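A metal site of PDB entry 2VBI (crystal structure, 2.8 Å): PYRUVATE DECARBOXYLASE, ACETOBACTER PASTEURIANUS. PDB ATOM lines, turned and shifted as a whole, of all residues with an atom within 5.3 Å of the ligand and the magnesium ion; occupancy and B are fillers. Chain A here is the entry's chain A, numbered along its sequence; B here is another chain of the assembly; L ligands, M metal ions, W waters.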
ATOM      1  N   GLU A 383       9.949 -10.134 -23.540  1.00  0.00           N
ATOM      2  CA  GLU A 383       9.980  -8.850 -22.853  1.00  0.00           C
ATOM      3  C   GLU A 383       8.696  -8.544 -22.084  1.00  0.00           C
ATOM      4  O   GLU A 383       7.619  -9.059 -22.416  1.00  0.00           O
ATOM      5  CB  GLU A 383      10.269  -7.734 -23.868  1.00  0.00           C
ATOM      6  CG  GLU A 383      10.378  -6.345 -23.280  1.00  0.00           C
ATOM      7  CD  GLU A 383      11.530  -6.201 -22.323  1.00  0.00           C
ATOM      8  OE1 GLU A 383      11.384  -6.591 -21.145  1.00  0.00           O
ATOM      9  OE2 GLU A 383      12.592  -5.692 -22.762  1.00  0.00           O
ATOM     10  N   THR A 384       8.824  -7.690 -21.066  1.00  0.00           N
ATOM     11  CA  THR A 384       7.682  -7.116 -20.369  1.00  0.00           C
ATOM     12  C   THR A 384       6.794  -6.367 -21.372  1.00  0.00           C
ATOM     13  O   THR A 384       7.277  -5.611 -22.211  1.00  0.00           O
ATOM     14  CB  THR A 384       8.133  -6.180 -19.246  1.00  0.00           C
ATOM     15  OG1 THR A 384       9.014  -6.890 -18.363  1.00  0.00           O
ATOM     16  CG2 THR A 384       6.939  -5.659 -18.441  1.00  0.00           C
ATOM     17  N   GLY A 385       5.491  -6.601 -21.270  1.00  0.00           N
ATOM     18  CA  GLY A 385       4.512  -6.095 -22.238  1.00  0.00           C
ATOM     19  C   GLY A 385       3.668  -7.262 -22.686  1.00  0.00           C
ATOM     20  O   GLY A 385       3.653  -8.311 -22.032  1.00  0.00           O
ATOM     21  N   ASP A 386       2.979  -7.115 -23.811  1.00  0.00           N
ATOM     22  CA  ASP A 386       2.119  -8.190 -24.307  1.00  0.00           C
ATOM     23  C   ASP A 386       2.912  -9.451 -24.669  1.00  0.00           C
ATOM     24  O   ASP A 386       2.332 -10.534 -24.789  1.00  0.00           O
ATOM     25  CB  ASP A 386       1.259  -7.710 -25.499  1.00  0.00           C
ATOM     26  CG  ASP A 386       0.039  -8.597 -25.743  1.00  0.00           C
ATOM     27  OD1 ASP A 386      -0.468  -9.207 -24.772  1.00  0.00           O
ATOM     28  OD2 ASP A 386      -0.428  -8.680 -26.913  1.00  0.00           O
ATOM     29  N   SER A 387       4.222  -9.321 -24.815  1.00  0.00           N
ATOM     30  CA  SER A 387       5.068 -10.473 -25.101  1.00  0.00           C
ATOM     31  C   SER A 387       5.077 -11.493 -23.956  1.00  0.00           C
ATOM     32  O   SER A 387       5.250 -12.680 -24.203  1.00  0.00           O
ATOM     33  CB  SER A 387       6.489 -10.047 -25.458  1.00  0.00           C
ATOM     34  OG  SER A 387       6.474  -9.204 -26.587  1.00  0.00           O
ATOM     35  N   GLY A 409      10.949  -6.712 -14.062  1.00  0.00           N
ATOM     36  CA  GLY A 409      10.090  -6.111 -15.102  1.00  0.00           C
ATOM     37  C   GLY A 409      10.551  -4.780 -15.676  1.00  0.00           C
ATOM     38  O   GLY A 409       9.748  -3.864 -15.851  1.00  0.00           O
ATOM     39  N   HIS A 410      11.852  -4.679 -15.951  1.00  0.00           N
ATOM     40  CA  HIS A 410      12.455  -3.490 -16.519  1.00  0.00           C
ATOM     41  C   HIS A 410      12.361  -3.586 -18.035  1.00  0.00           C
ATOM     42  O   HIS A 410      13.112  -4.371 -18.644  1.00  0.00           O
ATOM     43  CB  HIS A 410      13.931  -3.424 -16.107  1.00  0.00           C
ATOM     44  CG  HIS A 410      14.632  -2.176 -16.521  1.00  0.00           C
ATOM     45  ND1 HIS A 410      14.870  -1.851 -17.846  1.00  0.00           N
ATOM     46  CD2 HIS A 410      15.169  -1.164 -15.789  1.00  0.00           C
ATOM     47  CE1 HIS A 410      15.507  -0.696 -17.910  1.00  0.00           C
ATOM     48  NE2 HIS A 410      15.714  -0.263 -16.680  1.00  0.00           N
ATOM     49  N   ILE A 411      11.475  -2.817 -18.655  1.00  0.00           N
ATOM     50  CA  ILE A 411      11.380  -2.836 -20.116  1.00  0.00           C
ATOM     51  C   ILE A 411      12.720  -2.486 -20.761  1.00  0.00           C
ATOM     52  O   ILE A 411      13.477  -1.670 -20.249  1.00  0.00           O
ATOM     53  CB  ILE A 411      10.250  -1.909 -20.661  1.00  0.00           C
ATOM     54  CG1 ILE A 411      10.526  -0.448 -20.337  1.00  0.00           C
ATOM     55  CG2 ILE A 411       8.880  -2.358 -20.139  1.00  0.00           C
ATOM     56  CD1 ILE A 411       9.643   0.518 -21.078  1.00  0.00           C
ATOM     57  N   VAL A 434      10.098  -8.642 -28.410  1.00  0.00           N
ATOM     58  CA  VAL A 434      10.244  -7.338 -27.772  1.00  0.00           C
ATOM     59  C   VAL A 434       9.295  -6.315 -28.374  1.00  0.00           C
ATOM     60  O   VAL A 434       9.151  -6.239 -29.581  1.00  0.00           O
ATOM     61  CB  VAL A 434      11.720  -6.838 -27.789  1.00  0.00           C
ATOM     62  CG1 VAL A 434      12.225  -6.624 -29.197  1.00  0.00           C
ATOM     63  CG2 VAL A 434      11.886  -5.566 -26.968  1.00  0.00           C
ATOM     64  N   GLY A 435       8.649  -5.536 -27.509  1.00  0.00           N
ATOM     65  CA  GLY A 435       7.744  -4.482 -27.962  1.00  0.00           C
ATOM     66  C   GLY A 435       8.510  -3.278 -28.430  1.00  0.00           C
ATOM     67  O   GLY A 435       9.693  -3.118 -28.142  1.00  0.00           O
ATOM     68  N   ASP A 436       7.817  -2.407 -29.176  1.00  0.00           N
ATOM     69  CA  ASP A 436       8.450  -1.225 -29.734  1.00  0.00           C
ATOM     70  C   ASP A 436       8.892  -0.252 -28.641  1.00  0.00           C
ATOM     71  O   ASP A 436       9.960   0.349 -28.738  1.00  0.00           O
ATOM     72  CB  ASP A 436       7.559  -0.545 -30.787  1.00  0.00           C
ATOM     73  CG  ASP A 436       6.175  -0.149 -30.251  1.00  0.00           C
ATOM     74  OD1 ASP A 436       5.642  -0.824 -29.353  1.00  0.00           O
ATOM     75  OD2 ASP A 436       5.625   0.839 -30.768  1.00  0.00           O
ATOM     76  N   GLY A 437       8.077  -0.129 -27.598  1.00  0.00           N
ATOM     77  CA  GLY A 437       8.383   0.766 -26.494  1.00  0.00           C
ATOM     78  C   GLY A 437       9.615   0.332 -25.737  1.00  0.00           C
ATOM     79  O   GLY A 437      10.464   1.145 -25.379  1.00  0.00           O
ATOM     80  N   SER A 438       9.694  -0.979 -25.485  1.00  0.00           N
ATOM     81  CA  SER A 438      10.823  -1.544 -24.752  1.00  0.00           C
ATOM     82  C   SER A 438      12.114  -1.425 -25.530  1.00  0.00           C
ATOM     83  O   SER A 438      13.163  -1.132 -24.961  1.00  0.00           O
ATOM     84  CB  SER A 438      10.558  -3.018 -24.424  1.00  0.00           C
ATOM     85  OG  SER A 438       9.381  -3.157 -23.645  1.00  0.00           O
ATOM     86  N   PHE A 439      12.020  -1.661 -26.831  1.00  0.00           N
ATOM     87  CA  PHE A 439      13.187  -1.669 -27.679  1.00  0.00           C
ATOM     88  C   PHE A 439      13.925  -0.344 -27.615  1.00  0.00           C
ATOM     89  O   PHE A 439      15.157  -0.321 -27.637  1.00  0.00           O
ATOM     90  CB  PHE A 439      12.798  -2.010 -29.113  1.00  0.00           C
ATOM     91  CG  PHE A 439      13.958  -2.234 -30.026  1.00  0.00           C
ATOM     92  CD1 PHE A 439      14.652  -3.435 -30.012  1.00  0.00           C
ATOM     93  CD2 PHE A 439      14.367  -1.244 -30.905  1.00  0.00           C
ATOM     94  CE1 PHE A 439      15.734  -3.650 -30.863  1.00  0.00           C
ATOM     95  CE2 PHE A 439      15.449  -1.445 -31.759  1.00  0.00           C
ATOM     96  CZ  PHE A 439      16.139  -2.652 -31.737  1.00  0.00           C
ATOM     97  N   LEU A 441      14.515   1.710 -25.228  1.00  0.00           N
ATOM     98  CA  LEU A 441      15.382   1.913 -24.060  1.00  0.00           C
ATOM     99  C   LEU A 441      16.801   1.408 -24.237  1.00  0.00           C
ATOM    100  O   LEU A 441      17.741   1.999 -23.718  1.00  0.00           O
ATOM    101  CB  LEU A 441      14.794   1.259 -22.818  1.00  0.00           C
ATOM    102  CG  LEU A 441      13.698   2.035 -22.089  1.00  0.00           C
ATOM    103  CD1 LEU A 441      12.333   1.773 -22.705  1.00  0.00           C
ATOM    104  CD2 LEU A 441      13.699   1.665 -20.631  1.00  0.00           C
ATOM    105  N   ILE A 461       7.750  -6.239 -31.985  1.00  0.00           N
ATOM    106  CA  ILE A 461       6.296  -6.074 -32.104  1.00  0.00           C
ATOM    107  C   ILE A 461       5.944  -4.583 -32.120  1.00  0.00           C
ATOM    108  O   ILE A 461       5.801  -3.950 -31.070  1.00  0.00           O
ATOM    109  CB  ILE A 461       5.503  -6.810 -30.978  1.00  0.00           C
ATOM    110  CG1 ILE A 461       6.114  -8.185 -30.653  1.00  0.00           C
ATOM    111  CG2 ILE A 461       4.018  -6.903 -31.347  1.00  0.00           C
ATOM    112  CD1 ILE A 461       6.067  -9.226 -31.779  1.00  0.00           C
ATOM    113  N   ASN A 463       3.425  -2.119 -32.347  1.00  0.00           N
ATOM    114  CA  ASN A 463       2.001  -1.789 -32.244  1.00  0.00           C
ATOM    115  C   ASN A 463       1.760  -0.318 -31.907  1.00  0.00           C
ATOM    116  O   ASN A 463       0.657   0.065 -31.537  1.00  0.00           O
ATOM    117  CB  ASN A 463       1.273  -2.724 -31.280  1.00  0.00           C
ATOM    118  CG  ASN A 463       1.931  -2.801 -29.910  1.00  0.00           C
ATOM    119  OD1 ASN A 463       2.714  -1.934 -29.519  1.00  0.00           O
ATOM    120  ND2 ASN A 463       1.595  -3.837 -29.161  1.00  0.00           N
ATOM    121  N   ARG A 464       2.816   0.494 -32.030  1.00  0.00           N
ATOM    122  CA  ARG A 464       2.751   1.948 -31.897  1.00  0.00           C
ATOM    123  C   ARG A 464       2.465   2.470 -30.494  1.00  0.00           C
ATOM    124  O   ARG A 464       1.673   3.405 -30.323  1.00  0.00           O
ATOM    125  CB  ARG A 464       1.730   2.546 -32.885  1.00  0.00           C
ATOM    126  CG  ARG A 464       2.007   2.269 -34.329  1.00  0.00           C
ATOM    127  CD  ARG A 464       3.254   2.995 -34.804  1.00  0.00           C
ATOM    128  NE  ARG A 464       3.315   2.957 -36.259  1.00  0.00           N
ATOM    129  CZ  ARG A 464       3.010   3.981 -37.055  1.00  0.00           C
ATOM    130  NH1 ARG A 464       2.638   5.137 -36.530  1.00  0.00           N
ATOM    131  NH2 ARG A 464       3.098   3.841 -38.372  1.00  0.00           N
ATOM    132  N   GLY A 465       3.117   1.876 -29.493  1.00  0.00           N
ATOM    133  CA  GLY A 465       3.023   2.381 -28.130  1.00  0.00           C
ATOM    134  C   GLY A 465       3.037   1.342 -27.035  1.00  0.00           C
ATOM    135  O   GLY A 465       3.222   0.148 -27.282  1.00  0.00           O
ATOM    136  N   TYR A 466       2.848   1.842 -25.813  1.00  0.00           N
ATOM    137  CA  TYR A 466       2.803   1.024 -24.615  1.00  0.00           C
ATOM    138  C   TYR A 466       1.404   0.422 -24.492  1.00  0.00           C
ATOM    139  O   TYR A 466       0.573   0.904 -23.728  1.00  0.00           O
ATOM    140  CB  TYR A 466       3.097   1.863 -23.372  1.00  0.00           C
ATOM    141  CG  TYR A 466       4.435   2.605 -23.333  1.00  0.00           C
ATOM    142  CD1 TYR A 466       5.546   2.127 -24.029  1.00  0.00           C
ATOM    143  CD2 TYR A 466       4.575   3.760 -22.555  1.00  0.00           C
ATOM    144  CE1 TYR A 466       6.775   2.793 -23.965  1.00  0.00           C
ATOM    145  CE2 TYR A 466       5.801   4.434 -22.486  1.00  0.00           C
ATOM    146  CZ  TYR A 466       6.885   3.940 -23.193  1.00  0.00           C
ATOM    147  OH  TYR A 466       8.095   4.591 -23.135  1.00  0.00           O
ATOM    148  N   VAL A 467       1.151  -0.632 -25.265  1.00  0.00           N
ATOM    149  CA  VAL A 467      -0.200  -1.214 -25.366  1.00  0.00           C
ATOM    150  C   VAL A 467      -0.679  -1.843 -24.056  1.00  0.00           C
ATOM    151  O   VAL A 467      -1.847  -1.674 -23.684  1.00  0.00           O
ATOM    152  CB  VAL A 467      -0.316  -2.181 -26.564  1.00  0.00           C
ATOM    153  CG1 VAL A 467      -1.562  -3.054 -26.456  1.00  0.00           C
ATOM    154  CG2 VAL A 467      -0.349  -1.394 -27.846  1.00  0.00           C
ATOM    155  N   ILE A 468       0.226  -2.544 -23.352  1.00  0.00           N
ATOM    156  CA  ILE A 468      -0.080  -3.113 -22.035  1.00  0.00           C
ATOM    157  C   ILE A 468      -0.648  -2.046 -21.101  1.00  0.00           C
ATOM    158  O   ILE A 468      -1.368  -2.362 -20.154  1.00  0.00           O
ATOM    159  CB  ILE A 468       1.156  -3.788 -21.382  1.00  0.00           C
ATOM    160  CG1 ILE A 468       0.761  -4.519 -20.090  1.00  0.00           C
ATOM    161  CG2 ILE A 468       2.250  -2.757 -21.135  1.00  0.00           C
ATOM    162  CD1 ILE A 468       1.795  -5.517 -19.589  1.00  0.00           C
ATOM    163  N   GLU A 469      -0.337  -0.798 -21.397  1.00  0.00           N
ATOM    164  CA  GLU A 469      -0.750   0.325 -20.573  1.00  0.00           C
ATOM    165  C   GLU A 469      -1.964   1.006 -21.160  1.00  0.00           C
ATOM    166  O   GLU A 469      -2.856   1.434 -20.423  1.00  0.00           O
ATOM    167  CB  GLU A 469       0.402   1.302 -20.430  1.00  0.00           C
ATOM    168  CG  GLU A 469       0.587   1.807 -19.015  1.00  0.00           C
ATOM    169  CD  GLU A 469       1.024   0.703 -18.029  1.00  0.00           C
ATOM    170  OE1 GLU A 469       0.148   0.224 -17.257  1.00  0.00           O
ATOM    171  OE2 GLU A 469       2.243   0.345 -18.038  1.00  0.00           O
ATOM    172  N   VAL B  24       8.685   9.254 -17.681  1.00  0.00           N
ATOM    173  CA  VAL B  24       8.490   7.977 -18.336  1.00  0.00           C
ATOM    174  C   VAL B  24       7.397   7.245 -17.570  1.00  0.00           C
ATOM    175  O   VAL B  24       7.486   7.097 -16.333  1.00  0.00           O
ATOM    176  CB  VAL B  24       9.763   7.120 -18.357  1.00  0.00           C
ATOM    177  CG1 VAL B  24       9.514   5.800 -19.054  1.00  0.00           C
ATOM    178  CG2 VAL B  24      10.891   7.869 -19.042  1.00  0.00           C
ATOM    179  N   ALA B  25       6.370   6.801 -18.288  1.00  0.00           N
ATOM    180  CA  ALA B  25       5.192   6.183 -17.677  1.00  0.00           C
ATOM    181  C   ALA B  25       5.488   4.818 -17.074  1.00  0.00           C
ATOM    182  O   ALA B  25       6.310   4.067 -17.587  1.00  0.00           O
ATOM    183  CB  ALA B  25       4.075   6.063 -18.681  1.00  0.00           C
ATOM    184  N   GLY B  26       4.820   4.507 -15.968  1.00  0.00           N
ATOM    185  CA  GLY B  26       4.824   3.189 -15.377  1.00  0.00           C
ATOM    186  C   GLY B  26       3.627   3.086 -14.477  1.00  0.00           C
ATOM    187  O   GLY B  26       3.126   4.108 -13.989  1.00  0.00           O
ATOM    188  N   ASP B  27       3.162   1.873 -14.215  1.00  0.00           N
ATOM    189  CA  ASP B  27       1.910   1.710 -13.462  1.00  0.00           C
ATOM    190  C   ASP B  27       1.906   2.404 -12.081  1.00  0.00           C
ATOM    191  O   ASP B  27       0.860   2.916 -11.646  1.00  0.00           O
ATOM    192  CB  ASP B  27       1.439   0.240 -13.412  1.00  0.00           C
ATOM    193  CG  ASP B  27       2.405  -0.677 -12.663  1.00  0.00           C
ATOM    194  OD1 ASP B  27       3.600  -0.333 -12.488  1.00  0.00           O
ATOM    195  OD2 ASP B  27       1.958  -1.771 -12.256  1.00  0.00           O
ATOM    196  N   GLU B  50      14.863   6.236 -18.490  1.00  0.00           N
ATOM    197  CA  GLU B  50      14.943   7.032 -17.285  1.00  0.00           C
ATOM    198  C   GLU B  50      16.290   7.700 -17.059  1.00  0.00           C
ATOM    199  O   GLU B  50      16.355   8.776 -16.450  1.00  0.00           O
ATOM    200  CB  GLU B  50      14.537   6.205 -16.067  1.00  0.00           C
ATOM    201  CG  GLU B  50      13.055   5.850 -16.057  1.00  0.00           C
ATOM    202  CD  GLU B  50      12.699   4.610 -16.865  1.00  0.00           C
ATOM    203  OE1 GLU B  50      13.612   3.997 -17.486  1.00  0.00           O
ATOM    204  OE2 GLU B  50      11.507   4.247 -16.869  1.00  0.00           O
ATOM    205  N   THR B  72       8.993   5.670 -12.607  1.00  0.00           N
ATOM    206  CA  THR B  72       8.368   4.594 -11.865  1.00  0.00           C
ATOM    207  C   THR B  72       9.368   3.949 -10.894  1.00  0.00           C
ATOM    208  O   THR B  72      10.583   4.101 -11.055  1.00  0.00           O
ATOM    209  CB  THR B  72       7.729   3.540 -12.806  1.00  0.00           C
ATOM    210  OG1 THR B  72       6.851   2.696 -12.044  1.00  0.00           O
ATOM    211  CG2 THR B  72       8.782   2.713 -13.513  1.00  0.00           C
ATOM    212  N   VAL B  75      12.852   0.254 -11.190  1.00  0.00           N
ATOM    213  CA  VAL B  75      13.303   0.050 -12.566  1.00  0.00           C
ATOM    214  C   VAL B  75      13.532   1.389 -13.282  1.00  0.00           C
ATOM    215  O   VAL B  75      14.442   1.505 -14.110  1.00  0.00           O
ATOM    216  CB  VAL B  75      12.367  -0.887 -13.367  1.00  0.00           C
ATOM    217  CG1 VAL B  75      12.439  -2.283 -12.786  1.00  0.00           C
ATOM    218  CG2 VAL B  75      10.936  -0.388 -13.384  1.00  0.00           C
ATOM    219  N   GLY B  76      12.732   2.379 -12.931  1.00  0.00           N
ATOM    220  CA  GLY B  76      12.940   3.727 -13.414  1.00  0.00           C
ATOM    221  C   GLY B  76      13.912   4.487 -12.525  1.00  0.00           C
ATOM    222  O   GLY B  76      14.947   4.980 -12.976  1.00  0.00           O
ATOM    223  N   HIS B 114       8.709  -4.854  -9.587  1.00  0.00           N
ATOM    224  CA  HIS B 114       9.727  -3.799  -9.609  1.00  0.00           C
ATOM    225  C   HIS B 114      10.481  -3.664  -8.280  1.00  0.00           C
ATOM    226  O   HIS B 114      11.066  -2.623  -7.990  1.00  0.00           O
ATOM    227  CB  HIS B 114       9.168  -2.423 -10.013  1.00  0.00           C
ATOM    228  CG  HIS B 114       8.510  -2.398 -11.354  1.00  0.00           C
ATOM    229  ND1 HIS B 114       8.765  -3.325 -12.336  1.00  0.00           N
ATOM    230  CD2 HIS B 114       7.625  -1.522 -11.884  1.00  0.00           C
ATOM    231  CE1 HIS B 114       8.038  -3.041 -13.409  1.00  0.00           C
ATOM    232  NE2 HIS B 114       7.340  -1.948 -13.160  1.00  0.00           N
HETATM  233  N1  LIG L   1      10.217   2.049 -17.180  1.00  0.00           N
HETATM  234  C1  LIG L   1      10.997   0.904 -17.060  1.00  0.00           C
HETATM  235  C2  LIG L   1      12.487   1.026 -17.073  1.00  0.00           C
HETATM  236  N2  LIG L   1      10.397  -0.336 -16.946  1.00  0.00           N
HETATM  237  C3  LIG L   1       9.019  -0.442 -16.934  1.00  0.00           C
HETATM  238  N3  LIG L   1       8.485  -1.644 -16.802  1.00  0.00           N
HETATM  239  C4  LIG L   1       8.235   0.711 -17.050  1.00  0.00           C
HETATM  240  C5  LIG L   1       8.839   1.957 -17.171  1.00  0.00           C
HETATM  241  C6  LIG L   1       6.721   0.668 -17.044  1.00  0.00           C
HETATM  242  N4  LIG L   1       6.204  -0.072 -18.178  1.00  0.00           N
HETATM  243  C7  LIG L   1       5.762  -1.379 -18.077  1.00  0.00           C
HETATM  244  S1  LIG L   1       5.253  -1.980 -19.463  1.00  0.00           S
HETATM  245  C8  LIG L   1       5.545  -0.625 -20.257  1.00  0.00           C
HETATM  246  C9  LIG L   1       6.057   0.388 -19.457  1.00  0.00           C
HETATM  247  C10 LIG L   1       6.416   1.759 -19.971  1.00  0.00           C
HETATM  248  C11 LIG L   1       5.169  -0.647 -21.721  1.00  0.00           C
HETATM  249  C12 LIG L   1       6.061  -1.492 -22.635  1.00  0.00           C
HETATM  250  O1  LIG L   1       5.559  -1.344 -23.947  1.00  0.00           O
HETATM  251  P1  LIG L   1       6.020  -2.229 -25.223  1.00  0.00           P
HETATM  252  O2  LIG L   1       5.722  -1.445 -26.474  1.00  0.00           O
HETATM  253  O3  LIG L   1       7.487  -2.569 -25.168  1.00  0.00           O
HETATM  254  O4  LIG L   1       5.147  -3.579 -25.197  1.00  0.00           O
HETATM  255  P2  LIG L   1       3.573  -3.626 -25.576  1.00  0.00           P
HETATM  256  O5  LIG L   1       2.709  -3.293 -24.382  1.00  0.00           O
HETATM  257  O6  LIG L   1       3.263  -5.036 -26.038  1.00  0.00           O
HETATM  258  O7  LIG L   1       3.237  -2.640 -26.676  1.00  0.00           O
HETATM  259 MG    MG M   1       4.522  -1.581 -28.052  1.00  0.00          MG
HETATM  260  O   HOH W   1       4.480  -4.080 -28.372  1.00  0.00           O
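Merely in contact with the ligand: Gly 385 (3.9 Å), His 410 (3.5 Å), Gly 435 (3.4 Å), Leu 441 (3.8 Å), Tyr 466 (3.5 Å), Glu 469 (3.9 Å), Ala 25 of chain B (3.3 Å), Gly 26 of chain B (3.6 Å), Thr 72 of chain B (3.7 Å), Val 75 of chain B (3.6 Å) and His 114 of chain B (3.7 Å).
Hydrophobic or aromatic side chains that line the ligand: His 410, Ile 411, Leu 441, Tyr 466, Val 467, Ile 468, Val 75 of chain B and His 114 of chain B.
Of the 32 residues printed, 22 come within 4 Å of the ligand.
Along chain A the residues within 4 Å of the ligand span positions 385 to 469.
Gly 437 touches the magnesium ion (N to MG, 3.9 Å).
The backbone NH (N) of Asp 436 is in hydrogen-bond range of the backbone carbonyl oxygen (O) of Ile 461 (3.2 Å).
N of Arg 464 is in hydrogen-bond range of OD2 of Asp 436.
A ring nitrogen (NE2) of His 410 sits close to the backbone carbonyl oxygen of Val 75 of chain B (3.4 Å).
Water W1 lies within hydrogen-bond range of an oxygen (O6) of the ligand (2.8 Å), the side-chain amide nitrogen of Asn 463 (3.0 Å) and the backbone carbonyl oxygen of Ile 461 (3.0 Å).
The magnesium ion is bound by the side-chain carboxylate (OD1) of Asp 436 (1.9 Å), an oxygen (O2) of the ligand (2.0 Å), an oxygen (O7) of the ligand (2.2 Å), the backbone carbonyl oxygen (O) of Gly 465 (2.3 Å), the side-chain amide oxygen (OD1) of Asn 463 (2.4 Å) and water W1 (2.5 Å).
The magnesium ion has six donor atoms within binding distance.
The backbone NH (N) of Gly 437 sits at hydrogen-bond distance from an oxygen (O3) of the ligand, at 3.5 Å.
The backbone carbonyl oxygen of Gly 409 is in hydrogen-bond range of a nitrogen (N3) of the ligand.
The backbone NH (N) of Ser 438 lies within hydrogen-bond range of an oxygen (O3) of the ligand (2.7 Å).
The backbone NH (N) of Ile 468 is in hydrogen-bond range of an oxygen (O5) of the ligand, 2.8 Å away.
O6 of the ligand sits at hydrogen-bond distance from N of Asp 386 (3.1 Å).
O5 of the ligand sits at hydrogen-bond distance from N of Val 467, at 3.2 Å.
The side-chain hydroxyl (OG) of Ser 438 is in hydrogen-bond range of an oxygen (O3) of the ligand (2.5 Å).
A nitrogen (N1) of the ligand sits at hydrogen-bond distance from the side-chain carboxylate of Glu 50 of chain B.
N of Ile 411 lies within hydrogen-bond range of N2 of the ligand, at 3.2 Å.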
